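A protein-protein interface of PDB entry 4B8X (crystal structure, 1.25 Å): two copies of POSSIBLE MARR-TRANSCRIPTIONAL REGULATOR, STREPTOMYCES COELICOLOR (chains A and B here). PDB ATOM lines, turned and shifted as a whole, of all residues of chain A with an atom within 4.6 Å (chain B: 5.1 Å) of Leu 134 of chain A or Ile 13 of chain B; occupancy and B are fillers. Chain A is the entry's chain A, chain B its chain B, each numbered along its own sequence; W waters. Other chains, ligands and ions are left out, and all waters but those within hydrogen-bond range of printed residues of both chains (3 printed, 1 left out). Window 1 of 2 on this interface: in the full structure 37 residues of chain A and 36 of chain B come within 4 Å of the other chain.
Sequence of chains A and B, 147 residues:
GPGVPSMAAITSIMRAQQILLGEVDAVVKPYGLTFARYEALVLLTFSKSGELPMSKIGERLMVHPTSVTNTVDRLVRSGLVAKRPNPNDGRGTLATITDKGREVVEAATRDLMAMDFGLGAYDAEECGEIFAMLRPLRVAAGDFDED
O of Met 133 of chain A lies within hydrogen-bond range of OH of Tyr 122 of chain B. N of Leu 137 of chain A sits at hydrogen-bond distance from OH of Tyr 122 of chain B, 3.1 Å away. The guanidinium group (NH1) of Arg 138 of chain A sits at hydrogen-bond distance from the side-chain hydroxyl (OG) of Ser 12 of chain B.
NH1 of Arg 15 of chain B is in hydrogen-bond range of OE1 of Gln 18 of chain B, 2.9 Å away.
CG2 of Ile 13 of chain A touches CB of Ala 16 of chain B (3.97 Å). Gln 17 of chain B touches Gln 17 of chain A (CD to CD, 3.7 Å). Leu 20 of chain A touches Ile 13 of chain B. Ile 130 of chain A touches Ala 9 of chain B (CG2 to CB, 3.995 Å). CG1 of Ile 13 of chain B touches CG2 of Ile 130 of chain A, at 3.9 Å. Ser 12 of chain B touches Phe 131 of chain A. Met 133 of chain A touches Ile 130 of chain B (SD to CA, 3.8 Å). Leu 134 of chain A touches Tyr 122 of chain B (CA to OH, 3.6 Å). CG2 of Thr 11 of chain B touches NH2 of Arg 138 of chain A, at 3.9 Å. NE of Arg 138 of chain A touches CB of Arg 15 of chain B, 3.7 Å away.
Printed residues of chain B within 4 Å of Leu 134 of chain A: Ser 12 (3.5 Å), Ile 13 (3.8 Å) and Tyr 122 (3.6 Å). Of chain A, only Ala 16, Gln 17, Leu 20, Ile 130 and Leu 134 come within 4 Å of Ile 13 of chain B. Of the printed residues of chain A, Ser 12 of chain B touches Phe 131, Leu 134 and Arg 138. Printed residues of chain B within 4 Å of Leu 20 of chain A: Ile 10 (3.9996 Å) and Ile 13 (3.6 Å). Printed residues of chain B within 4 Å of Met 133 of chain A: Tyr 122 (2.8 Å), Ile 130 (3.8 Å) and Leu 134 (3.99 Å). Of the printed residues of chain A, Ile 130 of chain B touches Ile 13 and Met 133. Printed residues of chain A within 4 Å of Arg 15 of chain B: Arg 138 (3.7 Å). Gln 18 of chain B touches none of the printed residues of chain A. Arg 135 of chain A touches none of the printed residues of chain B. The nearest residue of chain A that does not touch Ile 13 of chain B is Ile 13 of chain A (4.2 Å). The nearest printed residue of chain A that does not touch Thr 11 of chain B is Leu 134 of chain A (6.6 Å).
Of the 13 printed residues of chain A, 11 touch a printed residue of chain B. Hydrophobic or aromatic side chains of chain A that line the printed part of chain B: Ile 13, Ala 16, Leu 20, Ile 130, Phe 131, Met 133, Leu 134, Pro 136 and Leu 137. Among the printed residues, no Asp or Glu carboxylate lies within 4 Å of a Lys or Arg side-chain nitrogen of the other chain.
Ile 13 of chain A touches Gln 17 of chain B, and with the chains exchanged Gln 17 of chain A touches Ile 13 of chain B. Ile 13 of chain A touches Ile 130 of chain B, and with the chains exchanged Ile 130 of chain A touches Ile 13 of chain B. Ile 13 of chain A touches Leu 134 of chain B, and with the chains exchanged Leu 134 of chain A touches Ile 13 of chain B. Gln 17 of chain B touches its own counterpart, Gln 17 of chain A. Positions printed for both chains: 13, 16, 17, 130 and 134. Of the 25 pairs that touch across the chains among the printed residues, 9 have their exchanged pair printed and touching as well.
Water W1 lies within hydrogen-bond range of the side-chain amide oxygen of Gln 17 of chain B (2.7 Å), the backbone carbonyl oxygen of Met 14 of chain B (2.8 Å) and the side-chain amide nitrogen of Gln 17 of chain A (3.2 Å). Water W2 lies within hydrogen-bond range of OG of Ser 12 of chain B (2.7 Å), O of Phe 131 of chain A (2.8 Å), NH1 of Arg 138 of chain A (3.2 Å) and N of Arg 135 of chain A (3.4 Å). Water W3 lies within hydrogen-bond range of OE1 of Gln 17 of chain A (2.8 Å) and NE2 of Gln 17 of chain B (3.1 Å).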
ATOM      1  N   ILE A  13       6.908 -21.936 -18.181  1.00  0.00           N
ATOM      2  CA  ILE A  13       8.346 -21.707 -18.271  1.00  0.00           C
ATOM      3  C   ILE A  13       8.826 -21.846 -19.720  1.00  0.00           C
ATOM      4  O   ILE A  13       9.622 -21.025 -20.191  1.00  0.00           O
ATOM      5  CB  ILE A  13       9.089 -22.676 -17.314  1.00  0.00           C
ATOM      6  CG1 ILE A  13       8.863 -22.264 -15.855  1.00  0.00           C
ATOM      7  CG2 ILE A  13      10.569 -22.694 -17.659  1.00  0.00           C
ATOM      8  CD1 ILE A  13       9.167 -23.342 -14.846  1.00  0.00           C
ATOM      9  N   ALA A  16       7.538 -18.820 -21.676  1.00  0.00           N
ATOM     10  CA  ALA A  16       8.238 -17.603 -21.313  1.00  0.00           C
ATOM     11  C   ALA A  16       9.628 -17.589 -21.930  1.00  0.00           C
ATOM     12  O   ALA A  16      10.088 -16.554 -22.431  1.00  0.00           O
ATOM     13  CB  ALA A  16       8.316 -17.460 -19.797  1.00  0.00           C
ATOM     14  N   GLN A  17      10.313 -18.719 -21.903  1.00  0.00           N
ATOM     15  CA  GLN A  17      11.650 -18.784 -22.460  1.00  0.00           C
ATOM     16  C   GLN A  17      11.615 -18.503 -23.966  1.00  0.00           C
ATOM     17  O   GLN A  17      12.480 -17.796 -24.479  1.00  0.00           O
ATOM     18  CB  GLN A  17      12.282 -20.140 -22.151  1.00  0.00           C
ATOM     19  CG  GLN A  17      13.727 -20.237 -22.608  1.00  0.00           C
ATOM     20  CD  GLN A  17      13.937 -20.802 -23.993  1.00  0.00           C
ATOM     21  OE1 GLN A  17      13.026 -21.238 -24.650  1.00  0.00           O
ATOM     22  NE2 GLN A  17      15.189 -20.790 -24.434  1.00  0.00           N
ATOM     23  N   LEU A  20      10.838 -14.680 -24.584  1.00  0.00           N
ATOM     24  CA  LEU A  20      11.971 -13.823 -24.282  1.00  0.00           C
ATOM     25  C   LEU A  20      13.140 -14.076 -25.230  1.00  0.00           C
ATOM     26  O   LEU A  20      13.794 -13.122 -25.667  1.00  0.00           O
ATOM     27  CB  LEU A  20      12.406 -14.001 -22.820  1.00  0.00           C
ATOM     28  CG  LEU A  20      11.377 -13.552 -21.791  1.00  0.00           C
ATOM     29  CD1 LEU A  20      11.903 -13.845 -20.388  1.00  0.00           C
ATOM     30  CD2 LEU A  20      11.018 -12.098 -21.949  1.00  0.00           C
ATOM     31  N   ILE A 130       9.765 -13.563  -9.956  1.00  0.00           N
ATOM     32  CA  ILE A 130      10.168 -14.570 -10.939  1.00  0.00           C
ATOM     33  C   ILE A 130      11.499 -15.210 -10.527  1.00  0.00           C
ATOM     34  O   ILE A 130      11.650 -16.432 -10.497  1.00  0.00           O
ATOM     35  CB  ILE A 130      10.234 -13.961 -12.343  1.00  0.00           C
ATOM     36  CG1 ILE A 130       8.797 -13.668 -12.832  1.00  0.00           C
ATOM     37  CG2 ILE A 130      10.989 -14.884 -13.294  1.00  0.00           C
ATOM     38  CD1 ILE A 130       8.686 -12.783 -14.050  1.00  0.00           C
ATOM     39  N   PHE A 131      12.462 -14.359 -10.148  1.00  0.00           N
ATOM     40  CA  PHE A 131      13.751 -14.827  -9.646  1.00  0.00           C
ATOM     41  C   PHE A 131      13.538 -15.731  -8.424  1.00  0.00           C
ATOM     42  O   PHE A 131      14.055 -16.829  -8.321  1.00  0.00           O
ATOM     43  CB  PHE A 131      14.689 -13.636  -9.338  1.00  0.00           C
ATOM     44  CG  PHE A 131      15.936 -14.039  -8.623  1.00  0.00           C
ATOM     45  CD1 PHE A 131      17.002 -14.545  -9.346  1.00  0.00           C
ATOM     46  CD2 PHE A 131      16.021 -13.989  -7.246  1.00  0.00           C
ATOM     47  CE1 PHE A 131      18.150 -14.968  -8.697  1.00  0.00           C
ATOM     48  CE2 PHE A 131      17.164 -14.424  -6.590  1.00  0.00           C
ATOM     49  CZ  PHE A 131      18.220 -14.911  -7.317  1.00  0.00           C
ATOM     50  N   ALA A 132      12.792 -15.231  -7.454  1.00  0.00           N
ATOM     51  CA  ALA A 132      12.649 -15.942  -6.206  1.00  0.00           C
ATOM     52  C   ALA A 132      11.927 -17.281  -6.378  1.00  0.00           C
ATOM     53  O   ALA A 132      12.283 -18.267  -5.719  1.00  0.00           O
ATOM     54  CB  ALA A 132      11.925 -15.072  -5.196  1.00  0.00           C
ATOM     55  N   MET A 133      10.922 -17.344  -7.247  1.00  0.00           N
ATOM     56  CA  MET A 133      10.128 -18.555  -7.406  1.00  0.00           C
ATOM     57  C   MET A 133      10.896 -19.678  -8.093  1.00  0.00           C
ATOM     58  O   MET A 133      10.636 -20.863  -7.829  1.00  0.00           O
ATOM     59  CB  MET A 133       8.797 -18.250  -8.133  1.00  0.00           C
ATOM     60  CG  MET A 133       8.864 -18.076  -9.646  1.00  0.00           C
ATOM     61  SD  MET A 133       7.399 -17.369 -10.480  1.00  0.00           S
ATOM     62  CE  MET A 133       7.996 -17.688 -12.130  1.00  0.00           C
ATOM     63  N   LEU A 134      11.854 -19.323  -8.949  1.00  0.00           N
ATOM     64  CA  LEU A 134      12.613 -20.311  -9.697  1.00  0.00           C
ATOM     65  C   LEU A 134      13.932 -20.664  -9.013  1.00  0.00           C
ATOM     66  O   LEU A 134      14.634 -21.593  -9.444  1.00  0.00           O
ATOM     67  CB  LEU A 134      12.871 -19.805 -11.109  1.00  0.00           C
ATOM     68  CG  LEU A 134      11.611 -19.582 -11.964  1.00  0.00           C
ATOM     69  CD1 LEU A 134      11.981 -18.952 -13.301  1.00  0.00           C
ATOM     70  CD2 LEU A 134      10.838 -20.889 -12.132  1.00  0.00           C
ATOM     71  N   ARG A 135      14.250 -19.942  -7.940  1.00  0.00           N
ATOM     72  CA  ARG A 135      15.544 -20.128  -7.276  1.00  0.00           C
ATOM     73  C   ARG A 135      15.738 -21.556  -6.724  1.00  0.00           C
ATOM     74  O   ARG A 135      16.794 -22.138  -6.912  1.00  0.00           O
ATOM     75  CB  ARG A 135      15.808 -19.046  -6.212  1.00  0.00           C
ATOM     76  CG  ARG A 135      17.284 -18.908  -5.848  1.00  0.00           C
ATOM     77  CD  ARG A 135      17.486 -17.869  -4.775  1.00  0.00           C
ATOM     78  NE  ARG A 135      18.894 -17.667  -4.445  1.00  0.00           N
ATOM     79  CZ  ARG A 135      19.588 -18.450  -3.637  1.00  0.00           C
ATOM     80  NH1 ARG A 135      19.026 -19.497  -3.053  1.00  0.00           N
ATOM     81  NH2 ARG A 135      20.867 -18.166  -3.406  1.00  0.00           N
ATOM     82  N   PRO A 136      14.712 -22.141  -6.069  1.00  0.00           N
ATOM     83  CA  PRO A 136      14.941 -23.489  -5.489  1.00  0.00           C
ATOM     84  C   PRO A 136      15.264 -24.548  -6.562  1.00  0.00           C
ATOM     85  O   PRO A 136      16.065 -25.453  -6.352  1.00  0.00           O
ATOM     86  CB  PRO A 136      13.634 -23.760  -4.741  1.00  0.00           C
ATOM     87  CG  PRO A 136      13.151 -22.392  -4.341  1.00  0.00           C
ATOM     88  CD  PRO A 136      13.461 -21.551  -5.563  1.00  0.00           C
ATOM     89  N   LEU A 137      14.608 -24.471  -7.713  1.00  0.00           N
ATOM     90  CA  LEU A 137      14.922 -25.350  -8.826  1.00  0.00           C
ATOM     91  C   LEU A 137      16.392 -25.237  -9.253  1.00  0.00           C
ATOM     92  O   LEU A 137      17.083 -26.234  -9.529  1.00  0.00           O
ATOM     93  CB  LEU A 137      13.969 -25.033 -10.000  1.00  0.00           C
ATOM     94  CG  LEU A 137      14.016 -25.975 -11.201  1.00  0.00           C
ATOM     95  CD1 LEU A 137      13.332 -27.297 -10.871  1.00  0.00           C
ATOM     96  CD2 LEU A 137      13.339 -25.329 -12.391  1.00  0.00           C
ATOM     97  N   ARG A 138      16.863 -24.000  -9.308  1.00  0.00           N
ATOM     98  CA  ARG A 138      18.248 -23.726  -9.655  1.00  0.00           C
ATOM     99  C   ARG A 138      19.243 -24.165  -8.585  1.00  0.00           C
ATOM    100  O   ARG A 138      20.308 -24.664  -8.918  1.00  0.00           O
ATOM    101  CB  ARG A 138      18.425 -22.245  -9.974  1.00  0.00           C
ATOM    102  CG  ARG A 138      17.678 -21.824 -11.216  1.00  0.00           C
ATOM    103  CD  ARG A 138      17.851 -20.370 -11.512  1.00  0.00           C
ATOM    104  NE  ARG A 138      19.244 -20.097 -11.777  1.00  0.00           N
ATOM    105  CZ  ARG A 138      19.762 -18.881 -11.716  1.00  0.00           C
ATOM    106  NH1 ARG A 138      18.993 -17.835 -11.388  1.00  0.00           N
ATOM    107  NH2 ARG A 138      21.049 -18.704 -11.975  1.00  0.00           N
ATOM    108  N   ALA B   9      15.767 -12.078 -13.675  1.00  0.00           N
ATOM    109  CA  ALA B   9      14.566 -12.788 -14.090  1.00  0.00           C
ATOM    110  C   ALA B   9      14.782 -13.566 -15.393  1.00  0.00           C
ATOM    111  O   ALA B   9      14.389 -14.736 -15.481  1.00  0.00           O
ATOM    112  CB  ALA B   9      13.393 -11.818 -14.179  1.00  0.00           C
ATOM    113  N   ILE B  10      15.387 -12.948 -16.415  1.00  0.00           N
ATOM    114  CA  ILE B  10      15.584 -13.686 -17.662  1.00  0.00           C
ATOM    115  C   ILE B  10      16.529 -14.861 -17.431  1.00  0.00           C
ATOM    116  O   ILE B  10      16.290 -15.944 -17.953  1.00  0.00           O
ATOM    117  CB  ILE B  10      16.037 -12.816 -18.861  1.00  0.00           C
ATOM    118  CG1 ILE B  10      15.890 -13.613 -20.171  1.00  0.00           C
ATOM    119  CG2 ILE B  10      17.443 -12.249 -18.673  1.00  0.00           C
ATOM    120  CD1 ILE B  10      16.103 -12.800 -21.438  1.00  0.00           C
ATOM    121  N   THR B  11      17.587 -14.657 -16.656  1.00  0.00           N
ATOM    122  CA  THR B  11      18.496 -15.757 -16.351  1.00  0.00           C
ATOM    123  C   THR B  11      17.757 -16.910 -15.676  1.00  0.00           C
ATOM    124  O   THR B  11      17.981 -18.083 -15.984  1.00  0.00           O
ATOM    125  CB  THR B  11      19.662 -15.276 -15.486  1.00  0.00           C
ATOM    126  OG1 THR B  11      20.400 -14.310 -16.233  1.00  0.00           O
ATOM    127  CG2 THR B  11      20.584 -16.447 -15.104  1.00  0.00           C
ATOM    128  N   SER B  12      16.892 -16.571 -14.734  1.00  0.00           N
ATOM    129  CA  SER B  12      16.136 -17.573 -14.018  1.00  0.00           C
ATOM    130  C   SER B  12      15.223 -18.388 -14.928  1.00  0.00           C
ATOM    131  O   SER B  12      15.124 -19.612 -14.789  1.00  0.00           O
ATOM    132  CB  SER B  12      15.292 -16.927 -12.933  1.00  0.00           C
ATOM    133  OG  SER B  12      16.135 -16.385 -11.947  1.00  0.00           O
ATOM    134  N   ILE B  13      14.532 -17.693 -15.842  1.00  0.00           N
ATOM    135  CA  ILE B  13      13.628 -18.363 -16.784  1.00  0.00           C
ATOM    136  C   ILE B  13      14.427 -19.260 -17.725  1.00  0.00           C
ATOM    137  O   ILE B  13      14.029 -20.400 -17.985  1.00  0.00           O
ATOM    138  CB  ILE B  13      12.782 -17.341 -17.561  1.00  0.00           C
ATOM    139  CG1 ILE B  13      11.759 -16.690 -16.627  1.00  0.00           C
ATOM    140  CG2 ILE B  13      12.130 -17.967 -18.794  1.00  0.00           C
ATOM    141  CD1 ILE B  13      11.170 -15.414 -17.175  1.00  0.00           C
ATOM    142  N   MET B  14      15.553 -18.743 -18.240  1.00  0.00           N
ATOM    143  CA  MET B  14      16.414 -19.495 -19.149  1.00  0.00           C
ATOM    144  C   MET B  14      16.928 -20.765 -18.477  1.00  0.00           C
ATOM    145  O   MET B  14      16.904 -21.863 -19.064  1.00  0.00           O
ATOM    146  CB  MET B  14      17.602 -18.633 -19.618  1.00  0.00           C
ATOM    147  CG  MET B  14      17.242 -17.460 -20.535  1.00  0.00           C
ATOM    148  SD  MET B  14      16.723 -17.949 -22.190  1.00  0.00           S
ATOM    149  CE  MET B  14      15.904 -16.465 -22.790  1.00  0.00           C
ATOM    150  N   ARG B  15      17.421 -20.609 -17.252  1.00  0.00           N
ATOM    151  CA  ARG B  15      17.928 -21.772 -16.518  1.00  0.00           C
ATOM    152  C   ARG B  15      16.827 -22.769 -16.220  1.00  0.00           C
ATOM    153  O   ARG B  15      17.040 -23.982 -16.361  1.00  0.00           O
ATOM    154  CB  ARG B  15      18.637 -21.351 -15.224  1.00  0.00           C
ATOM    155  CG  ARG B  15      20.016 -20.734 -15.434  1.00  0.00           C
ATOM    156  CD  ARG B  15      21.004 -21.744 -15.969  1.00  0.00           C
ATOM    157  NE  ARG B  15      21.150 -22.879 -15.056  1.00  0.00           N
ATOM    158  CZ  ARG B  15      21.185 -24.168 -15.395  1.00  0.00           C
ATOM    159  NH1 ARG B  15      21.028 -24.564 -16.644  1.00  0.00           N
ATOM    160  NH2 ARG B  15      21.339 -25.084 -14.462  1.00  0.00           N
ATOM    161  N   ALA B  16      15.669 -22.292 -15.753  1.00  0.00           N
ATOM    162  CA  ALA B  16      14.591 -23.214 -15.455  1.00  0.00           C
ATOM    163  C   ALA B  16      14.195 -24.010 -16.694  1.00  0.00           C
ATOM    164  O   ALA B  16      13.927 -25.200 -16.591  1.00  0.00           O
ATOM    165  CB  ALA B  16      13.392 -22.466 -14.872  1.00  0.00           C
ATOM    166  N   GLN B  17      14.123 -23.347 -17.838  1.00  0.00           N
ATOM    167  CA  GLN B  17      13.770 -24.047 -19.066  1.00  0.00           C
ATOM    168  C   GLN B  17      14.820 -25.109 -19.418  1.00  0.00           C
ATOM    169  O   GLN B  17      14.453 -26.236 -19.785  1.00  0.00           O
ATOM    170  CB  GLN B  17      13.600 -23.034 -20.187  1.00  0.00           C
ATOM    171  CG  GLN B  17      13.111 -23.669 -21.473  1.00  0.00           C
ATOM    172  CD  GLN B  17      14.188 -24.111 -22.450  1.00  0.00           C
ATOM    173  OE1 GLN B  17      15.363 -23.906 -22.236  1.00  0.00           O
ATOM    174  NE2 GLN B  17      13.757 -24.674 -23.571  1.00  0.00           N
ATOM    175  N   GLN B  18      16.098 -24.781 -19.247  1.00  0.00           N
ATOM    176  CA  GLN B  18      17.154 -25.765 -19.556  1.00  0.00           C
ATOM    177  C   GLN B  18      17.091 -26.972 -18.612  1.00  0.00           C
ATOM    178  O   GLN B  18      17.237 -28.115 -19.036  1.00  0.00           O
ATOM    179  CB  GLN B  18      18.523 -25.132 -19.392  1.00  0.00           C
ATOM    180  CG  GLN B  18      19.016 -24.235 -20.507  1.00  0.00           C
ATOM    181  CD  GLN B  18      20.462 -23.760 -20.233  1.00  0.00           C
ATOM    182  OE1 GLN B  18      20.706 -23.144 -19.195  1.00  0.00           O
ATOM    183  NE2 GLN B  18      21.412 -24.022 -21.168  1.00  0.00           N
ATOM    184  N   TYR B 122       8.824 -29.329  -6.082  1.00  0.00           N
ATOM    185  CA  TYR B 122       7.996 -28.152  -5.815  1.00  0.00           C
ATOM    186  C   TYR B 122       6.656 -28.645  -5.282  1.00  0.00           C
ATOM    187  O   TYR B 122       6.216 -29.757  -5.572  1.00  0.00           O
ATOM    188  CB  TYR B 122       7.773 -27.320  -7.111  1.00  0.00           C
ATOM    189  CG  TYR B 122       8.863 -26.294  -7.391  1.00  0.00           C
ATOM    190  CD1 TYR B 122      10.206 -26.568  -7.154  1.00  0.00           C
ATOM    191  CD2 TYR B 122       8.538 -25.046  -7.842  1.00  0.00           C
ATOM    192  CE1 TYR B 122      11.178 -25.605  -7.370  1.00  0.00           C
ATOM    193  CE2 TYR B 122       9.507 -24.079  -8.070  1.00  0.00           C
ATOM    194  CZ  TYR B 122      10.813 -24.353  -7.815  1.00  0.00           C
ATOM    195  OH  TYR B 122      11.744 -23.373  -8.046  1.00  0.00           O
ATOM    196  N   ILE B 130       4.249 -20.069 -10.316  1.00  0.00           N
ATOM    197  CA  ILE B 130       4.948 -20.007 -11.587  1.00  0.00           C
ATOM    198  C   ILE B 130       3.967 -19.673 -12.715  1.00  0.00           C
ATOM    199  O   ILE B 130       4.180 -18.757 -13.514  1.00  0.00           O
ATOM    200  CB  ILE B 130       5.718 -21.295 -11.883  1.00  0.00           C
ATOM    201  CG1 ILE B 130       6.897 -21.434 -10.916  1.00  0.00           C
ATOM    202  CG2 ILE B 130       6.160 -21.323 -13.348  1.00  0.00           C
ATOM    203  CD1 ILE B 130       7.474 -22.833 -10.913  1.00  0.00           C
ATOM    204  N   LEU B 134       3.949 -15.885 -14.737  1.00  0.00           N
ATOM    205  CA  LEU B 134       4.352 -15.820 -16.137  1.00  0.00           C
ATOM    206  C   LEU B 134       3.148 -15.568 -17.066  1.00  0.00           C
ATOM    207  O   LEU B 134       3.314 -15.321 -18.259  1.00  0.00           O
ATOM    208  CB  LEU B 134       5.117 -17.067 -16.537  1.00  0.00           C
ATOM    209  CG  LEU B 134       6.422 -17.279 -15.776  1.00  0.00           C
ATOM    210  CD1 LEU B 134       7.073 -18.611 -16.135  1.00  0.00           C
ATOM    211  CD2 LEU B 134       7.398 -16.126 -16.017  1.00  0.00           C
HETATM  212  O   HOH W   1      16.916 -21.684 -21.873  1.00  0.00           O
HETATM  213  O   HOH W   2      16.302 -17.899  -9.661  1.00  0.00           O
HETATM  214  O   HOH W   3      11.148 -23.338 -24.484  1.00  0.00           O
